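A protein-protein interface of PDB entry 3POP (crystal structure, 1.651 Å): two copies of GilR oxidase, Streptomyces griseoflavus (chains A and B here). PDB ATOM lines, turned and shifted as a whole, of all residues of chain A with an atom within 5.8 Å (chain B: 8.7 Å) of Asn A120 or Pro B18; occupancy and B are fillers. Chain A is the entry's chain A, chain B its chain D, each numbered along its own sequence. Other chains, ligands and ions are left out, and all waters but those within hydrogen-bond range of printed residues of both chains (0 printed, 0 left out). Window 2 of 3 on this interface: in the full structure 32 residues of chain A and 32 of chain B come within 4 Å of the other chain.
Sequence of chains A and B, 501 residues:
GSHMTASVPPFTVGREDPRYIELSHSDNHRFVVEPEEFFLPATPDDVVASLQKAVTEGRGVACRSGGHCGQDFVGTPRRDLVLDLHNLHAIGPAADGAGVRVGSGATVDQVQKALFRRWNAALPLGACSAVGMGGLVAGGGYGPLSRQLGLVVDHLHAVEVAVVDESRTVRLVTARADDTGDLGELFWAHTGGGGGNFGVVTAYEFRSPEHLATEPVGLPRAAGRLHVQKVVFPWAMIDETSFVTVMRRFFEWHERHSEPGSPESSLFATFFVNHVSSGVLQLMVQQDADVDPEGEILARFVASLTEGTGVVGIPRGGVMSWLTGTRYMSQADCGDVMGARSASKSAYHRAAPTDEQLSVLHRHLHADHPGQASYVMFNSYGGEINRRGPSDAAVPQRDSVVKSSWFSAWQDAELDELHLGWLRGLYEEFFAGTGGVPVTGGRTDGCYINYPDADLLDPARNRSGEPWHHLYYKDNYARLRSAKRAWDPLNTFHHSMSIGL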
ATOM      1  N   LEU A 115       4.523 -26.013  -9.019  1.00  0.00           N
ATOM      2  CA  LEU A 115       4.663 -25.772 -10.454  1.00  0.00           C
ATOM      3  C   LEU A 115       5.618 -24.621 -10.729  1.00  0.00           C
ATOM      4  O   LEU A 115       6.434 -24.678 -11.646  1.00  0.00           O
ATOM      5  CB  LEU A 115       3.307 -25.461 -11.086  1.00  0.00           C
ATOM      6  CG  LEU A 115       2.564 -26.653 -11.710  1.00  0.00           C
ATOM      7  CD1 LEU A 115       2.753 -27.936 -10.948  1.00  0.00           C
ATOM      8  CD2 LEU A 115       1.094 -26.315 -11.890  1.00  0.00           C
ATOM      9  N   PHE A 116       5.500 -23.548  -9.948  1.00  0.00           N
ATOM     10  CA  PHE A 116       6.367 -22.408 -10.160  1.00  0.00           C
ATOM     11  C   PHE A 116       7.818 -22.709  -9.784  1.00  0.00           C
ATOM     12  O   PHE A 116       8.733 -22.468 -10.573  1.00  0.00           O
ATOM     13  CB  PHE A 116       5.915 -21.168  -9.393  1.00  0.00           C
ATOM     14  CG  PHE A 116       6.870 -20.025  -9.545  1.00  0.00           C
ATOM     15  CD1 PHE A 116       6.813 -19.214 -10.661  1.00  0.00           C
ATOM     16  CD2 PHE A 116       7.862 -19.802  -8.599  1.00  0.00           C
ATOM     17  CE1 PHE A 116       7.726 -18.176 -10.830  1.00  0.00           C
ATOM     18  CE2 PHE A 116       8.760 -18.772  -8.756  1.00  0.00           C
ATOM     19  CZ  PHE A 116       8.693 -17.957  -9.867  1.00  0.00           C
ATOM     20  N   ARG A 117       8.024 -23.222  -8.579  1.00  0.00           N
ATOM     21  CA  ARG A 117       9.371 -23.440  -8.068  1.00  0.00           C
ATOM     22  C   ARG A 117      10.161 -24.484  -8.856  1.00  0.00           C
ATOM     23  O   ARG A 117      11.371 -24.348  -9.031  1.00  0.00           O
ATOM     24  CB  ARG A 117       9.324 -23.807  -6.583  1.00  0.00           C
ATOM     25  CG  ARG A 117       8.453 -22.873  -5.760  1.00  0.00           C
ATOM     26  CD  ARG A 117       9.062 -22.582  -4.402  1.00  0.00           C
ATOM     27  NE  ARG A 117       8.500 -23.435  -3.361  1.00  0.00           N
ATOM     28  CZ  ARG A 117       7.987 -22.988  -2.220  1.00  0.00           C
ATOM     29  NH1 ARG A 117       7.962 -21.688  -1.963  1.00  0.00           N
ATOM     30  NH2 ARG A 117       7.499 -23.843  -1.334  1.00  0.00           N
ATOM     31  N   ARG A 118       9.482 -25.523  -9.333  1.00  0.00           N
ATOM     32  CA  ARG A 118      10.169 -26.603 -10.034  1.00  0.00           C
ATOM     33  C   ARG A 118      10.326 -26.374 -11.523  1.00  0.00           C
ATOM     34  O   ARG A 118      11.334 -26.768 -12.103  1.00  0.00           O
ATOM     35  CB  ARG A 118       9.491 -27.944  -9.773  1.00  0.00           C
ATOM     36  CG  ARG A 118       9.484 -28.313  -8.318  1.00  0.00           C
ATOM     37  CD  ARG A 118       8.822 -29.647  -8.082  1.00  0.00           C
ATOM     38  NE  ARG A 118       8.190 -29.678  -6.766  1.00  0.00           N
ATOM     39  CZ  ARG A 118       7.504 -30.713  -6.294  1.00  0.00           C
ATOM     40  NH1 ARG A 118       7.370 -31.799  -7.049  1.00  0.00           N
ATOM     41  NH2 ARG A 118       6.958 -30.659  -5.076  1.00  0.00           N
ATOM     42  N   TRP A 119       9.344 -25.732 -12.149  1.00  0.00           N
ATOM     43  CA  TRP A 119       9.299 -25.693 -13.604  1.00  0.00           C
ATOM     44  C   TRP A 119       8.961 -24.321 -14.164  1.00  0.00           C
ATOM     45  O   TRP A 119       8.782 -24.170 -15.373  1.00  0.00           O
ATOM     46  CB  TRP A 119       8.287 -26.734 -14.132  1.00  0.00           C
ATOM     47  CG  TRP A 119       8.586 -28.132 -13.685  1.00  0.00           C
ATOM     48  CD1 TRP A 119       9.683 -28.889 -14.019  1.00  0.00           C
ATOM     49  CD2 TRP A 119       7.789 -28.947 -12.822  1.00  0.00           C
ATOM     50  NE1 TRP A 119       9.615 -30.118 -13.406  1.00  0.00           N
ATOM     51  CE2 TRP A 119       8.463 -30.182 -12.666  1.00  0.00           C
ATOM     52  CE3 TRP A 119       6.582 -28.752 -12.146  1.00  0.00           C
ATOM     53  CZ2 TRP A 119       7.958 -31.216 -11.874  1.00  0.00           C
ATOM     54  CZ3 TRP A 119       6.086 -29.779 -11.358  1.00  0.00           C
ATOM     55  CH2 TRP A 119       6.770 -30.996 -11.230  1.00  0.00           C
ATOM     56  N   ASN A 120       8.876 -23.312 -13.304  1.00  0.00           N
ATOM     57  CA  ASN A 120       8.415 -22.007 -13.763  1.00  0.00           C
ATOM     58  C   ASN A 120       7.110 -22.166 -14.531  1.00  0.00           C
ATOM     59  O   ASN A 120       6.888 -21.497 -15.534  1.00  0.00           O
ATOM     60  CB  ASN A 120       9.483 -21.322 -14.644  1.00  0.00           C
ATOM     61  CG  ASN A 120       9.169 -19.865 -14.928  1.00  0.00           C
ATOM     62  OD1 ASN A 120       9.445 -19.354 -16.020  1.00  0.00           O
ATOM     63  ND2 ASN A 120       8.590 -19.179 -13.944  1.00  0.00           N
ATOM     64  N   ALA A 121       6.230 -23.041 -14.044  1.00  0.00           N
ATOM     65  CA  ALA A 121       4.982 -23.322 -14.751  1.00  0.00           C
ATOM     66  C   ALA A 121       3.796 -22.765 -13.994  1.00  0.00           C
ATOM     67  O   ALA A 121       3.926 -22.386 -12.829  1.00  0.00           O
ATOM     68  CB  ALA A 121       4.808 -24.809 -14.940  1.00  0.00           C
ATOM     69  N   ALA A 122       2.633 -22.732 -14.653  1.00  0.00           N
ATOM     70  CA  ALA A 122       1.401 -22.253 -14.018  1.00  0.00           C
ATOM     71  C   ALA A 122       0.196 -22.875 -14.692  1.00  0.00           C
ATOM     72  O   ALA A 122       0.185 -23.048 -15.911  1.00  0.00           O
ATOM     73  CB  ALA A 122       1.291 -20.740 -14.102  1.00  0.00           C
ATOM     74  N   PRO A 220       2.207 -24.620 -19.253  1.00  0.00           N
ATOM     75  CA  PRO A 220       2.448 -23.226 -19.633  1.00  0.00           C
ATOM     76  C   PRO A 220       3.530 -22.578 -18.769  1.00  0.00           C
ATOM     77  O   PRO A 220       3.804 -23.027 -17.664  1.00  0.00           O
ATOM     78  CB  PRO A 220       1.110 -22.542 -19.326  1.00  0.00           C
ATOM     79  CG  PRO A 220       0.104 -23.663 -19.239  1.00  0.00           C
ATOM     80  CD  PRO A 220       0.878 -24.795 -18.643  1.00  0.00           C
ATOM     81  N   ARG A 221       4.113 -21.501 -19.275  1.00  0.00           N
ATOM     82  CA  ARG A 221       5.114 -20.765 -18.516  1.00  0.00           C
ATOM     83  C   ARG A 221       4.418 -19.729 -17.635  1.00  0.00           C
ATOM     84  O   ARG A 221       3.542 -19.002 -18.096  1.00  0.00           O
ATOM     85  CB  ARG A 221       6.081 -20.075 -19.493  1.00  0.00           C
ATOM     86  CG  ARG A 221       7.126 -19.207 -18.832  1.00  0.00           C
ATOM     87  CD  ARG A 221       8.124 -18.632 -19.849  1.00  0.00           C
ATOM     88  NE  ARG A 221       7.463 -17.786 -20.843  1.00  0.00           N
ATOM     89  CZ  ARG A 221       7.215 -16.490 -20.669  1.00  0.00           C
ATOM     90  NH1 ARG A 221       6.604 -15.790 -21.616  1.00  0.00           N
ATOM     91  NH2 ARG A 221       7.579 -15.893 -19.539  1.00  0.00           N
ATOM     92  N   ALA A 222       4.807 -19.657 -16.366  1.00  0.00           N
ATOM     93  CA  ALA A 222       4.395 -18.568 -15.496  1.00  0.00           C
ATOM     94  C   ALA A 222       4.977 -17.239 -15.969  1.00  0.00           C
ATOM     95  O   ALA A 222       6.165 -17.153 -16.310  1.00  0.00           O
ATOM     96  CB  ALA A 222       4.842 -18.857 -14.069  1.00  0.00           C
ATOM     97  N   ALA A 223       4.165 -16.194 -15.982  1.00  0.00           N
ATOM     98  CA  ALA A 223       4.641 -14.873 -16.409  1.00  0.00           C
ATOM     99  C   ALA A 223       5.806 -14.409 -15.534  1.00  0.00           C
ATOM    100  O   ALA A 223       5.868 -14.704 -14.343  1.00  0.00           O
ATOM    101  CB  ALA A 223       3.505 -13.855 -16.360  1.00  0.00           C
ATOM    102  N   GLY A 224       6.748 -13.680 -16.118  1.00  0.00           N
ATOM    103  CA  GLY A 224       7.876 -13.218 -15.333  1.00  0.00           C
ATOM    104  C   GLY A 224       7.458 -12.209 -14.281  1.00  0.00           C
ATOM    105  O   GLY A 224       7.939 -12.230 -13.149  1.00  0.00           O
ATOM    106  N   PHE B  11      18.166 -28.727  -7.257  1.00  0.00           N
ATOM    107  CA  PHE B  11      18.523 -27.960  -8.444  1.00  0.00           C
ATOM    108  C   PHE B  11      18.992 -26.551  -8.108  1.00  0.00           C
ATOM    109  O   PHE B  11      18.873 -26.096  -6.974  1.00  0.00           O
ATOM    110  CB  PHE B  11      17.349 -27.900  -9.420  1.00  0.00           C
ATOM    111  CG  PHE B  11      16.126 -27.247  -8.855  1.00  0.00           C
ATOM    112  CD1 PHE B  11      15.854 -25.916  -9.118  1.00  0.00           C
ATOM    113  CD2 PHE B  11      15.248 -27.968  -8.061  1.00  0.00           C
ATOM    114  CE1 PHE B  11      14.726 -25.313  -8.599  1.00  0.00           C
ATOM    115  CE2 PHE B  11      14.117 -27.375  -7.534  1.00  0.00           C
ATOM    116  CZ  PHE B  11      13.854 -26.043  -7.803  1.00  0.00           C
ATOM    117  N   VAL B  13      19.245 -22.330  -9.260  1.00  0.00           N
ATOM    118  CA  VAL B  13      18.581 -21.247  -9.975  1.00  0.00           C
ATOM    119  C   VAL B  13      19.572 -20.091 -10.095  1.00  0.00           C
ATOM    120  O   VAL B  13      19.878 -19.418  -9.106  1.00  0.00           O
ATOM    121  CB  VAL B  13      17.331 -20.752  -9.224  1.00  0.00           C
ATOM    122  CG1 VAL B  13      16.728 -19.558  -9.930  1.00  0.00           C
ATOM    123  CG2 VAL B  13      16.297 -21.878  -9.088  1.00  0.00           C
ATOM    124  N   GLY B  14      20.069 -19.874 -11.309  1.00  0.00           N
ATOM    125  CA  GLY B  14      21.042 -18.831 -11.571  1.00  0.00           C
ATOM    126  C   GLY B  14      20.411 -17.511 -11.962  1.00  0.00           C
ATOM    127  O   GLY B  14      19.190 -17.377 -11.991  1.00  0.00           O
ATOM    128  N   ARG B  15      21.256 -16.532 -12.270  1.00  0.00           N
ATOM    129  CA  ARG B  15      20.800 -15.183 -12.580  1.00  0.00           C
ATOM    130  C   ARG B  15      19.965 -15.095 -13.855  1.00  0.00           C
ATOM    131  O   ARG B  15      19.185 -14.159 -14.020  1.00  0.00           O
ATOM    132  CB  ARG B  15      21.992 -14.227 -12.676  1.00  0.00           C
ATOM    133  CG  ARG B  15      22.593 -13.843 -11.334  1.00  0.00           C
ATOM    134  CD  ARG B  15      23.946 -13.173 -11.510  1.00  0.00           C
ATOM    135  NE  ARG B  15      24.474 -12.661 -10.249  1.00  0.00           N
ATOM    136  CZ  ARG B  15      24.203 -11.454  -9.763  1.00  0.00           C
ATOM    137  NH1 ARG B  15      24.726 -11.069  -8.608  1.00  0.00           N
ATOM    138  NH2 ARG B  15      23.407 -10.631 -10.431  1.00  0.00           N
ATOM    139  N   GLU B  16      20.127 -16.058 -14.757  1.00  0.00           N
ATOM    140  CA  GLU B  16      19.405 -16.021 -16.029  1.00  0.00           C
ATOM    141  C   GLU B  16      18.089 -16.799 -16.003  1.00  0.00           C
ATOM    142  O   GLU B  16      17.292 -16.708 -16.935  1.00  0.00           O
ATOM    143  CB  GLU B  16      20.294 -16.541 -17.163  1.00  0.00           C
ATOM    144  N   ASP B  17      17.880 -17.568 -14.939  1.00  0.00           N
ATOM    145  CA  ASP B  17      16.672 -18.384 -14.776  1.00  0.00           C
ATOM    146  C   ASP B  17      15.508 -17.470 -14.384  1.00  0.00           C
ATOM    147  O   ASP B  17      15.665 -16.586 -13.548  1.00  0.00           O
ATOM    148  CB  ASP B  17      16.950 -19.425 -13.696  1.00  0.00           C
ATOM    149  CG  ASP B  17      15.844 -20.455 -13.557  1.00  0.00           C
ATOM    150  OD1 ASP B  17      16.174 -21.661 -13.601  1.00  0.00           O
ATOM    151  OD2 ASP B  17      14.671 -20.064 -13.368  1.00  0.00           O
ATOM    152  N   PRO B  18      14.334 -17.659 -15.001  1.00  0.00           N
ATOM    153  CA  PRO B  18      13.209 -16.763 -14.710  1.00  0.00           C
ATOM    154  C   PRO B  18      12.747 -16.846 -13.253  1.00  0.00           C
ATOM    155  O   PRO B  18      12.104 -15.910 -12.785  1.00  0.00           O
ATOM    156  CB  PRO B  18      12.096 -17.273 -15.638  1.00  0.00           C
ATOM    157  CG  PRO B  18      12.784 -18.126 -16.652  1.00  0.00           C
ATOM    158  CD  PRO B  18      13.974 -18.712 -15.966  1.00  0.00           C
ATOM    159  N   ARG B  19      13.093 -17.921 -12.549  1.00  0.00           N
ATOM    160  CA  ARG B  19      12.640 -18.070 -11.152  1.00  0.00           C
ATOM    161  C   ARG B  19      13.481 -17.210 -10.217  1.00  0.00           C
ATOM    162  O   ARG B  19      13.152 -17.013  -9.055  1.00  0.00           O
ATOM    163  CB  ARG B  19      12.724 -19.526 -10.714  1.00  0.00           C
ATOM    164  CG  ARG B  19      11.718 -20.427 -11.441  1.00  0.00           C
ATOM    165  CD  ARG B  19      12.011 -21.876 -11.186  1.00  0.00           C
ATOM    166  NE  ARG B  19      13.206 -22.294 -11.907  1.00  0.00           N
ATOM    167  CZ  ARG B  19      13.737 -23.512 -11.826  1.00  0.00           C
ATOM    168  NH1 ARG B  19      13.180 -24.437 -11.055  1.00  0.00           N
ATOM    169  NH2 ARG B  19      14.831 -23.804 -12.519  1.00  0.00           N
ATOM    170  N   TYR B  20      14.585 -16.692 -10.732  1.00  0.00           N
ATOM    171  CA  TYR B  20      15.496 -15.925  -9.894  1.00  0.00           C
ATOM    172  C   TYR B  20      14.837 -14.688  -9.339  1.00  0.00           C
ATOM    173  O   TYR B  20      15.102 -14.315  -8.203  1.00  0.00           O
ATOM    174  CB  TYR B  20      16.729 -15.530 -10.706  1.00  0.00           C
ATOM    175  CG  TYR B  20      17.829 -14.824  -9.933  1.00  0.00           C
ATOM    176  CD1 TYR B  20      18.903 -15.534  -9.425  1.00  0.00           C
ATOM    177  CD2 TYR B  20      17.812 -13.453  -9.774  1.00  0.00           C
ATOM    178  CE1 TYR B  20      19.942 -14.891  -8.744  1.00  0.00           C
ATOM    179  CE2 TYR B  20      18.834 -12.795  -9.097  1.00  0.00           C
ATOM    180  CZ  TYR B  20      19.892 -13.526  -8.585  1.00  0.00           C
ATOM    181  OH  TYR B  20      20.922 -12.874  -7.930  1.00  0.00           O
ATOM    182  N   ILE B  21      13.983 -14.053 -10.139  1.00  0.00           N
ATOM    183  CA  ILE B  21      13.299 -12.832  -9.715  1.00  0.00           C
ATOM    184  C   ILE B  21      12.469 -13.049  -8.444  1.00  0.00           C
ATOM    185  O   ILE B  21      12.600 -12.292  -7.475  1.00  0.00           O
ATOM    186  CB  ILE B  21      12.375 -12.291 -10.816  1.00  0.00           C
ATOM    187  CG1 ILE B  21      13.192 -11.992 -12.066  1.00  0.00           C
ATOM    188  CG2 ILE B  21      11.715 -11.011 -10.350  1.00  0.00           C
ATOM    189  CD1 ILE B  21      14.347 -11.056 -11.787  1.00  0.00           C
ATOM    190  N   GLU B  22      11.632 -14.082  -8.441  1.00  0.00           N
ATOM    191  CA  GLU B  22      10.865 -14.419  -7.240  1.00  0.00           C
ATOM    192  C   GLU B  22      11.785 -14.734  -6.059  1.00  0.00           C
ATOM    193  O   GLU B  22      11.573 -14.248  -4.942  1.00  0.00           O
ATOM    194  CB  GLU B  22       9.885 -15.584  -7.529  1.00  0.00           C
ATOM    195  CG  GLU B  22       9.123 -16.059  -6.295  1.00  0.00           C
ATOM    196  CD  GLU B  22       8.108 -15.035  -5.800  1.00  0.00           C
ATOM    197  OE1 GLU B  22       7.952 -14.888  -4.562  1.00  0.00           O
ATOM    198  OE2 GLU B  22       7.449 -14.392  -6.651  1.00  0.00           O
ATOM    199  N   LEU B  23      12.826 -15.529  -6.293  1.00  0.00           N
ATOM    200  CA  LEU B  23      13.709 -15.922  -5.208  1.00  0.00           C
ATOM    201  C   LEU B  23      14.494 -14.742  -4.630  1.00  0.00           C
ATOM    202  O   LEU B  23      14.944 -14.781  -3.484  1.00  0.00           O
ATOM    203  CB  LEU B  23      14.648 -17.051  -5.643  1.00  0.00           C
ATOM    204  CG  LEU B  23      13.973 -18.400  -5.928  1.00  0.00           C
ATOM    205  CD1 LEU B  23      14.998 -19.447  -6.343  1.00  0.00           C
ATOM    206  CD2 LEU B  23      13.199 -18.894  -4.716  1.00  0.00           C
ATOM    207  N   SER B  24      14.652 -13.682  -5.410  1.00  0.00           N
ATOM    208  CA  SER B  24      15.484 -12.571  -4.967  1.00  0.00           C
ATOM    209  C   SER B  24      14.771 -11.707  -3.936  1.00  0.00           C
ATOM    210  O   SER B  24      15.339 -10.736  -3.436  1.00  0.00           O
ATOM    211  CB  SER B  24      15.921 -11.710  -6.160  1.00  0.00           C
ATOM    212  OG  SER B  24      14.829 -10.977  -6.686  1.00  0.00           O
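O of Leu A115 sits at hydrogen-bond distance from N of Asn A120 (3.3 Å).
The backbone carbonyl oxygen (O) of Ala A121 sits at hydrogen-bond distance from the backbone NH (N) of Phe A116 (3.5 Å).
The backbone carbonyl oxygen (O) of Asn A120 sits at hydrogen-bond distance from the backbone NH (N) of Ala A222 (2.9 Å).
The side-chain carboxylate of Asp B17 lies within salt-bridge range of the guanidinium group of Arg B19 (2.8 Å).
No position is printed for both chains.
Of the 6 pairs that touch across the chains among the printed residues, none has its exchanged pair printed and touching as well.
Hydrophobic or aromatic side chains of chain B that line the printed part of chain A: Phe B11 and Pro B18.
Along chain B the printed residues that touch a printed residue of chain A span positions 11 to 22.
Of the printed residues of chain B, Phe A116 touches Arg B19 and Glu B22.
Printed residues of chain B within 4 Å of Arg A118: Arg B19.
Trp A119 touches none of the printed residues of chain B.
Printed residues of chain B within 4 Å of Asn A120: Pro B18 (3.4 Å).
No residue of chain B comes within 4 Å of Ala A121.
Arg A221 touches none of the printed residues of chain B.
Of the printed residues of chain A, Phe B11 touches Arg A117 (3.2 Å).
Pro B18 touches just one residue of chain A: Asn A120 (3.4 Å).
Of the printed residues of chain A, Arg B19 touches Phe A116, Arg A117 and Arg A118.
Of the printed residues of chain A, Glu B22 touches Phe A116 (3.5 Å).
The nearest printed residue of chain B that does not touch Asn A120 is Arg B19 (4.01 Å).
The nearest residue of chain A that does not touch Pro B18 is Phe A116 (4.9 Å).
The nearest printed residue of chain A that does not touch Arg B19 is Asn A120 (4.01 Å).
O of Phe A116 touches CD of Arg B19, at 3.4 Å.
CB of Glu B22 touches CZ of Phe A116 (3.5 Å).
Arg A117 touches Phe B11 (O to CZ, 3.2 Å).
Pro B18 touches Asn A120.
The backbone carbonyl oxygen (O) of Arg A117 is in hydrogen-bond range of the guanidinium group (NH1) of Arg B19 (2.7 Å).
O of Arg A118 sits at hydrogen-bond distance from NH1 of Arg B19 (3.2 Å).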
